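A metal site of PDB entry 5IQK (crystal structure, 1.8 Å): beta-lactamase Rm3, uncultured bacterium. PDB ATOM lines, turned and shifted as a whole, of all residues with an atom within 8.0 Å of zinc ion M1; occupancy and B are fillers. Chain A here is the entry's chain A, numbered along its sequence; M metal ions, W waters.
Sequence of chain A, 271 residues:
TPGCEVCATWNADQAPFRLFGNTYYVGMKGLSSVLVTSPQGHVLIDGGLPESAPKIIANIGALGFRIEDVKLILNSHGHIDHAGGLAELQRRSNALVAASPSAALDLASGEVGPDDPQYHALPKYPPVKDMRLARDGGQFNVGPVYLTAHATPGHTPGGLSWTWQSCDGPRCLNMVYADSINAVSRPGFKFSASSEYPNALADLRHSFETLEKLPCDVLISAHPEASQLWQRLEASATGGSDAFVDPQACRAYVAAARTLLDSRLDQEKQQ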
ATOM      1  N   TRP A  10      12.213 -20.935  -2.612  1.00  0.00           N
ATOM      2  CA  TRP A  10      13.206 -21.938  -2.235  1.00  0.00           C
ATOM      3  C   TRP A  10      13.300 -22.124  -0.715  1.00  0.00           C
ATOM      4  O   TRP A  10      13.519 -23.239  -0.234  1.00  0.00           O
ATOM      5  CB  TRP A  10      14.576 -21.575  -2.787  1.00  0.00           C
ATOM      6  CG  TRP A  10      14.710 -21.789  -4.293  1.00  0.00           C
ATOM      7  CD1 TRP A  10      13.756 -22.279  -5.147  1.00  0.00           C
ATOM      8  CD2 TRP A  10      15.856 -21.500  -5.094  1.00  0.00           C
ATOM      9  NE1 TRP A  10      14.256 -22.321  -6.445  1.00  0.00           N
ATOM     10  CE2 TRP A  10      15.544 -21.853  -6.427  1.00  0.00           C
ATOM     11  CE3 TRP A  10      17.122 -20.967  -4.828  1.00  0.00           C
ATOM     12  CZ2 TRP A  10      16.455 -21.697  -7.478  1.00  0.00           C
ATOM     13  CZ3 TRP A  10      18.020 -20.813  -5.871  1.00  0.00           C
ATOM     14  CH2 TRP A  10      17.682 -21.182  -7.174  1.00  0.00           C
ATOM     15  N   GLY A  30      12.472 -25.773  -1.204  1.00  0.00           N
ATOM     16  CA  GLY A  30      13.222 -25.750  -2.463  1.00  0.00           C
ATOM     17  C   GLY A  30      14.708 -25.971  -2.328  1.00  0.00           C
ATOM     18  O   GLY A  30      15.430 -25.913  -3.340  1.00  0.00           O
ATOM     19  N   LEU A  31      15.179 -26.235  -1.104  1.00  0.00           N
ATOM     20  CA  LEU A  31      16.596 -26.432  -0.817  1.00  0.00           C
ATOM     21  C   LEU A  31      16.783 -27.535   0.224  1.00  0.00           C
ATOM     22  O   LEU A  31      16.233 -27.429   1.324  1.00  0.00           O
ATOM     23  CB  LEU A  31      17.218 -25.133  -0.288  1.00  0.00           C
ATOM     24  CG  LEU A  31      17.155 -23.919  -1.210  1.00  0.00           C
ATOM     25  CD1 LEU A  31      17.543 -22.665  -0.443  1.00  0.00           C
ATOM     26  CD2 LEU A  31      18.067 -24.138  -2.405  1.00  0.00           C
ATOM     27  N   SER A  32      17.572 -28.567  -0.089  1.00  0.00           N
ATOM     28  CA  SER A  32      17.677 -29.700   0.810  1.00  0.00           C
ATOM     29  C   SER A  32      18.716 -29.471   1.907  1.00  0.00           C
ATOM     30  O   SER A  32      19.682 -28.748   1.730  1.00  0.00           O
ATOM     31  CB  SER A  32      18.024 -30.981   0.051  1.00  0.00           C
ATOM     32  OG  SER A  32      16.993 -31.324  -0.866  1.00  0.00           O
ATOM     33  N   ASP A  46      24.574 -29.768   3.881  1.00  0.00           N
ATOM     34  CA  ASP A  46      24.176 -28.491   3.284  1.00  0.00           C
ATOM     35  C   ASP A  46      23.473 -27.551   4.260  1.00  0.00           C
ATOM     36  O   ASP A  46      22.922 -27.971   5.301  1.00  0.00           O
ATOM     37  CB  ASP A  46      23.306 -28.735   2.054  1.00  0.00           C
ATOM     38  CG  ASP A  46      24.118 -28.715   0.759  1.00  0.00           C
ATOM     39  OD1 ASP A  46      25.324 -28.387   0.830  1.00  0.00           O
ATOM     40  OD2 ASP A  46      23.533 -28.985  -0.305  1.00  0.00           O
ATOM     41  N   SER A  76      27.662 -29.498  -0.638  1.00  0.00           N
ATOM     42  CA  SER A  76      27.536 -30.010  -1.993  1.00  0.00           C
ATOM     43  C   SER A  76      28.299 -29.083  -2.957  1.00  0.00           C
ATOM     44  O   SER A  76      29.259 -29.497  -3.597  1.00  0.00           O
ATOM     45  CB  SER A  76      26.071 -30.120  -2.395  1.00  0.00           C
ATOM     46  OG  SER A  76      25.416 -28.873  -2.230  1.00  0.00           O
ATOM     47  N   HIS A  77      27.866 -27.827  -3.051  1.00  0.00           N
ATOM     48  CA  HIS A  77      28.652 -26.846  -3.816  1.00  0.00           C
ATOM     49  C   HIS A  77      28.517 -25.427  -3.246  1.00  0.00           C
ATOM     50  O   HIS A  77      27.685 -25.169  -2.378  1.00  0.00           O
ATOM     51  CB  HIS A  77      28.300 -26.880  -5.309  1.00  0.00           C
ATOM     52  CG  HIS A  77      26.901 -26.427  -5.665  1.00  0.00           C
ATOM     53  ND1 HIS A  77      25.797 -27.245  -5.527  1.00  0.00           N
ATOM     54  CD2 HIS A  77      26.453 -25.285  -6.247  1.00  0.00           C
ATOM     55  CE1 HIS A  77      24.720 -26.608  -5.961  1.00  0.00           C
ATOM     56  NE2 HIS A  77      25.089 -25.421  -6.398  1.00  0.00           N
ATOM     57  N   HIS A  79      27.522 -22.387  -4.166  1.00  0.00           N
ATOM     58  CA  HIS A  79      26.507 -21.361  -4.376  1.00  0.00           C
ATOM     59  C   HIS A  79      25.818 -20.972  -3.084  1.00  0.00           C
ATOM     60  O   HIS A  79      25.670 -21.812  -2.193  1.00  0.00           O
ATOM     61  CB  HIS A  79      25.475 -21.826  -5.391  1.00  0.00           C
ATOM     62  CG  HIS A  79      25.944 -21.771  -6.810  1.00  0.00           C
ATOM     63  ND1 HIS A  79      25.402 -22.565  -7.788  1.00  0.00           N
ATOM     64  CD2 HIS A  79      26.895 -21.008  -7.418  1.00  0.00           C
ATOM     65  CE1 HIS A  79      25.981 -22.292  -8.953  1.00  0.00           C
ATOM     66  NE2 HIS A  79      26.894 -21.363  -8.751  1.00  0.00           N
ATOM     67  N   ILE A  80      25.395 -19.718  -3.023  1.00  0.00           N
ATOM     68  CA  ILE A  80      24.785 -19.165  -1.818  1.00  0.00           C
ATOM     69  C   ILE A  80      23.568 -19.945  -1.310  1.00  0.00           C
ATOM     70  O   ILE A  80      23.298 -19.943  -0.104  1.00  0.00           O
ATOM     71  CB  ILE A  80      24.388 -17.664  -2.056  1.00  0.00           C
ATOM     72  CG1 ILE A  80      23.893 -17.011  -0.760  1.00  0.00           C
ATOM     73  CG2 ILE A  80      23.345 -17.543  -3.172  1.00  0.00           C
ATOM     74  CD1 ILE A  80      23.871 -15.481  -0.817  1.00  0.00           C
ATOM     75  N   ASP A  81      22.842 -20.618  -2.191  1.00  0.00           N
ATOM     76  CA  ASP A  81      21.639 -21.318  -1.744  1.00  0.00           C
ATOM     77  C   ASP A  81      21.934 -22.683  -1.125  1.00  0.00           C
ATOM     78  O   ASP A  81      20.990 -23.382  -0.722  1.00  0.00           O
ATOM     79  CB  ASP A  81      20.628 -21.483  -2.897  1.00  0.00           C
ATOM     80  CG  ASP A  81      21.224 -22.182  -4.114  1.00  0.00           C
ATOM     81  OD1 ASP A  81      22.379 -21.866  -4.452  1.00  0.00           O
ATOM     82  OD2 ASP A  81      20.537 -23.034  -4.737  1.00  0.00           O
ATOM     83  N   HIS A  82      23.217 -23.068  -1.046  1.00  0.00           N
ATOM     84  CA  HIS A  82      23.618 -24.304  -0.341  1.00  0.00           C
ATOM     85  C   HIS A  82      24.655 -23.993   0.745  1.00  0.00           C
ATOM     86  O   HIS A  82      24.761 -24.696   1.756  1.00  0.00           O
ATOM     87  CB  HIS A  82      24.150 -25.336  -1.352  1.00  0.00           C
ATOM     88  CG  HIS A  82      23.185 -25.614  -2.466  1.00  0.00           C
ATOM     89  ND1 HIS A  82      22.147 -26.517  -2.339  1.00  0.00           N
ATOM     90  CD2 HIS A  82      23.043 -25.048  -3.686  1.00  0.00           C
ATOM     91  CE1 HIS A  82      21.429 -26.519  -3.447  1.00  0.00           C
ATOM     92  NE2 HIS A  82      21.953 -25.636  -4.287  1.00  0.00           N
ATOM     93  N   ALA A  83      25.425 -22.928   0.527  1.00  0.00           N
ATOM     94  CA  ALA A  83      26.525 -22.599   1.415  1.00  0.00           C
ATOM     95  C   ALA A  83      26.263 -21.380   2.289  1.00  0.00           C
ATOM     96  O   ALA A  83      27.001 -21.140   3.242  1.00  0.00           O
ATOM     97  CB  ALA A  83      27.827 -22.397   0.593  1.00  0.00           C
ATOM     98  N   GLN A 118      27.773 -18.854 -12.493  1.00  0.00           N
ATOM     99  CA  GLN A 118      27.010 -17.726 -11.957  1.00  0.00           C
ATOM    100  C   GLN A 118      27.868 -16.669 -11.252  1.00  0.00           C
ATOM    101  O   GLN A 118      27.370 -15.878 -10.448  1.00  0.00           O
ATOM    102  CB  GLN A 118      25.916 -18.244 -11.037  1.00  0.00           C
ATOM    103  CG  GLN A 118      24.976 -19.192 -11.771  1.00  0.00           C
ATOM    104  CD  GLN A 118      23.833 -19.699 -10.916  1.00  0.00           C
ATOM    105  OE1 GLN A 118      23.611 -20.909 -10.824  1.00  0.00           O
ATOM    106  NE2 GLN A 118      23.092 -18.778 -10.307  1.00  0.00           N
ATOM    107  N   LEU A 122      25.502 -13.576  -8.282  1.00  0.00           N
ATOM    108  CA  LEU A 122      24.969 -14.009  -6.981  1.00  0.00           C
ATOM    109  C   LEU A 122      25.493 -13.091  -5.881  1.00  0.00           C
ATOM    110  O   LEU A 122      26.589 -12.544  -5.987  1.00  0.00           O
ATOM    111  CB  LEU A 122      25.337 -15.469  -6.703  1.00  0.00           C
ATOM    112  CG  LEU A 122      24.630 -16.555  -7.533  1.00  0.00           C
ATOM    113  CD1 LEU A 122      25.210 -17.939  -7.275  1.00  0.00           C
ATOM    114  CD2 LEU A 122      23.133 -16.547  -7.306  1.00  0.00           C
ATOM    115  N   HIS A 155      27.772 -28.203 -12.838  1.00  0.00           N
ATOM    116  CA  HIS A 155      26.927 -27.082 -12.450  1.00  0.00           C
ATOM    117  C   HIS A 155      27.816 -26.018 -11.798  1.00  0.00           C
ATOM    118  O   HIS A 155      27.573 -24.819 -11.959  1.00  0.00           O
ATOM    119  CB  HIS A 155      25.809 -27.561 -11.518  1.00  0.00           C
ATOM    120  CG  HIS A 155      25.041 -26.478 -10.842  1.00  0.00           C
ATOM    121  ND1 HIS A 155      23.971 -25.831 -11.433  1.00  0.00           N
ATOM    122  CD2 HIS A 155      25.153 -25.943  -9.598  1.00  0.00           C
ATOM    123  CE1 HIS A 155      23.477 -24.936 -10.603  1.00  0.00           C
ATOM    124  NE2 HIS A 155      24.164 -24.997  -9.466  1.00  0.00           N
ATOM    125  N   THR A 156      28.830 -26.469 -11.064  1.00  0.00           N
ATOM    126  CA  THR A 156      29.958 -25.630 -10.613  1.00  0.00           C
ATOM    127  C   THR A 156      31.223 -26.478 -10.722  1.00  0.00           C
ATOM    128  O   THR A 156      31.130 -27.705 -10.795  1.00  0.00           O
ATOM    129  CB  THR A 156      29.808 -25.141  -9.156  1.00  0.00           C
ATOM    130  OG1 THR A 156      29.907 -26.263  -8.263  1.00  0.00           O
ATOM    131  CG2 THR A 156      28.487 -24.422  -8.932  1.00  0.00           C
ATOM    132  N   ASP A 179      24.471 -33.798  -5.775  1.00  0.00           N
ATOM    133  CA  ASP A 179      24.597 -32.385  -6.040  1.00  0.00           C
ATOM    134  C   ASP A 179      23.813 -32.014  -7.295  1.00  0.00           C
ATOM    135  O   ASP A 179      23.491 -32.861  -8.130  1.00  0.00           O
ATOM    136  CB  ASP A 179      26.071 -31.991  -6.218  1.00  0.00           C
ATOM    137  CG  ASP A 179      26.258 -30.486  -6.165  1.00  0.00           C
ATOM    138  OD1 ASP A 179      25.348 -29.787  -5.639  1.00  0.00           O
ATOM    139  OD2 ASP A 179      27.291 -29.999  -6.659  1.00  0.00           O
ATOM    140  N   SER A 180      23.506 -30.731  -7.417  1.00  0.00           N
ATOM    141  CA  SER A 180      22.994 -30.179  -8.674  1.00  0.00           C
ATOM    142  C   SER A 180      23.921 -30.527  -9.827  1.00  0.00           C
ATOM    143  O   SER A 180      25.129 -30.377  -9.694  1.00  0.00           O
ATOM    144  CB  SER A 180      22.873 -28.656  -8.592  1.00  0.00           C
ATOM    145  OG  SER A 180      22.007 -28.279  -7.530  1.00  0.00           O
ATOM    146  N   ASN A 182      22.563 -29.576 -13.064  1.00  0.00           N
ATOM    147  CA  ASN A 182      21.832 -28.907 -14.127  1.00  0.00           C
ATOM    148  C   ASN A 182      22.663 -27.778 -14.741  1.00  0.00           C
ATOM    149  O   ASN A 182      23.248 -26.941 -14.043  1.00  0.00           O
ATOM    150  CB  ASN A 182      20.474 -28.389 -13.609  1.00  0.00           C
ATOM    151  CG  ASN A 182      20.589 -27.421 -12.418  1.00  0.00           C
ATOM    152  OD1 ASN A 182      21.471 -27.538 -11.568  1.00  0.00           O
ATOM    153  ND2 ASN A 182      19.657 -26.483 -12.342  1.00  0.00           N
ATOM    154  N   VAL A 184      22.689 -24.724 -15.833  1.00  0.00           N
ATOM    155  CA  VAL A 184      22.095 -23.400 -15.785  1.00  0.00           C
ATOM    156  C   VAL A 184      23.189 -22.430 -15.353  1.00  0.00           C
ATOM    157  O   VAL A 184      24.190 -22.836 -14.736  1.00  0.00           O
ATOM    158  CB  VAL A 184      20.921 -23.331 -14.795  1.00  0.00           C
ATOM    159  CG1 VAL A 184      19.873 -24.358 -15.163  1.00  0.00           C
ATOM    160  CG2 VAL A 184      21.422 -23.591 -13.374  1.00  0.00           C
ATOM    161  N   ALA A 222      20.083 -31.978  -4.151  1.00  0.00           N
ATOM    162  CA  ALA A 222      20.346 -30.689  -3.511  1.00  0.00           C
ATOM    163  C   ALA A 222      19.152 -29.756  -3.647  1.00  0.00           C
ATOM    164  O   ALA A 222      18.806 -29.038  -2.700  1.00  0.00           O
ATOM    165  CB  ALA A 222      21.604 -30.063  -4.102  1.00  0.00           C
ATOM    166  N   HIS A 223      18.511 -29.770  -4.808  1.00  0.00           N
ATOM    167  CA  HIS A 223      17.186 -29.153  -4.958  1.00  0.00           C
ATOM    168  C   HIS A 223      16.163 -30.292  -4.943  1.00  0.00           C
ATOM    169  O   HIS A 223      16.134 -31.085  -5.887  1.00  0.00           O
ATOM    170  CB  HIS A 223      17.093 -28.316  -6.249  1.00  0.00           C
ATOM    171  CG  HIS A 223      17.850 -27.029  -6.199  1.00  0.00           C
ATOM    172  ND1 HIS A 223      17.237 -25.798  -6.075  1.00  0.00           N
ATOM    173  CD2 HIS A 223      19.187 -26.784  -6.268  1.00  0.00           C
ATOM    174  CE1 HIS A 223      18.158 -24.853  -6.052  1.00  0.00           C
ATOM    175  NE2 HIS A 223      19.345 -25.423  -6.176  1.00  0.00           N
HETATM  176 ZN    ZN M   1      21.151 -24.589  -5.802  1.00  0.00          ZN
HETATM  177 ZN    ZN M   2      24.060 -24.106  -7.627  1.00  0.00          ZN
HETATM  178  O   HOH W   1      22.344 -23.463  -7.126  1.00  0.00           O
HETATM  179  O   HOH W   2      22.033 -25.701  -7.710  1.00  0.00           O
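A ring nitrogen (ND1) of His 82 lies within hydrogen-bond range of the side-chain carboxylate (OD2) of Asp 46 (3.5 Å).
A ring nitrogen (ND1) of His 223 lies within hydrogen-bond range of the backbone carbonyl oxygen (O) of Gly 30 (3.3 Å).
Three residues have an atom within 4 Å of zinc ion M1: Asp 81, His 82 and His 223.
Zinc ion M1 is bound by the side-chain carboxylate (OD2) of Asp 81, at 2.0 Å.
Zinc ion M1 is bound by a ring nitrogen (NE2) of His 82 (2.0 Å).
NE2 of His 223 is bound to zinc ion M1, 2.0 Å away.
Zinc ion M1 is bound by water W1 (2.1 Å).
Zinc ion M1 is bound by water W2, at 2.4 Å.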
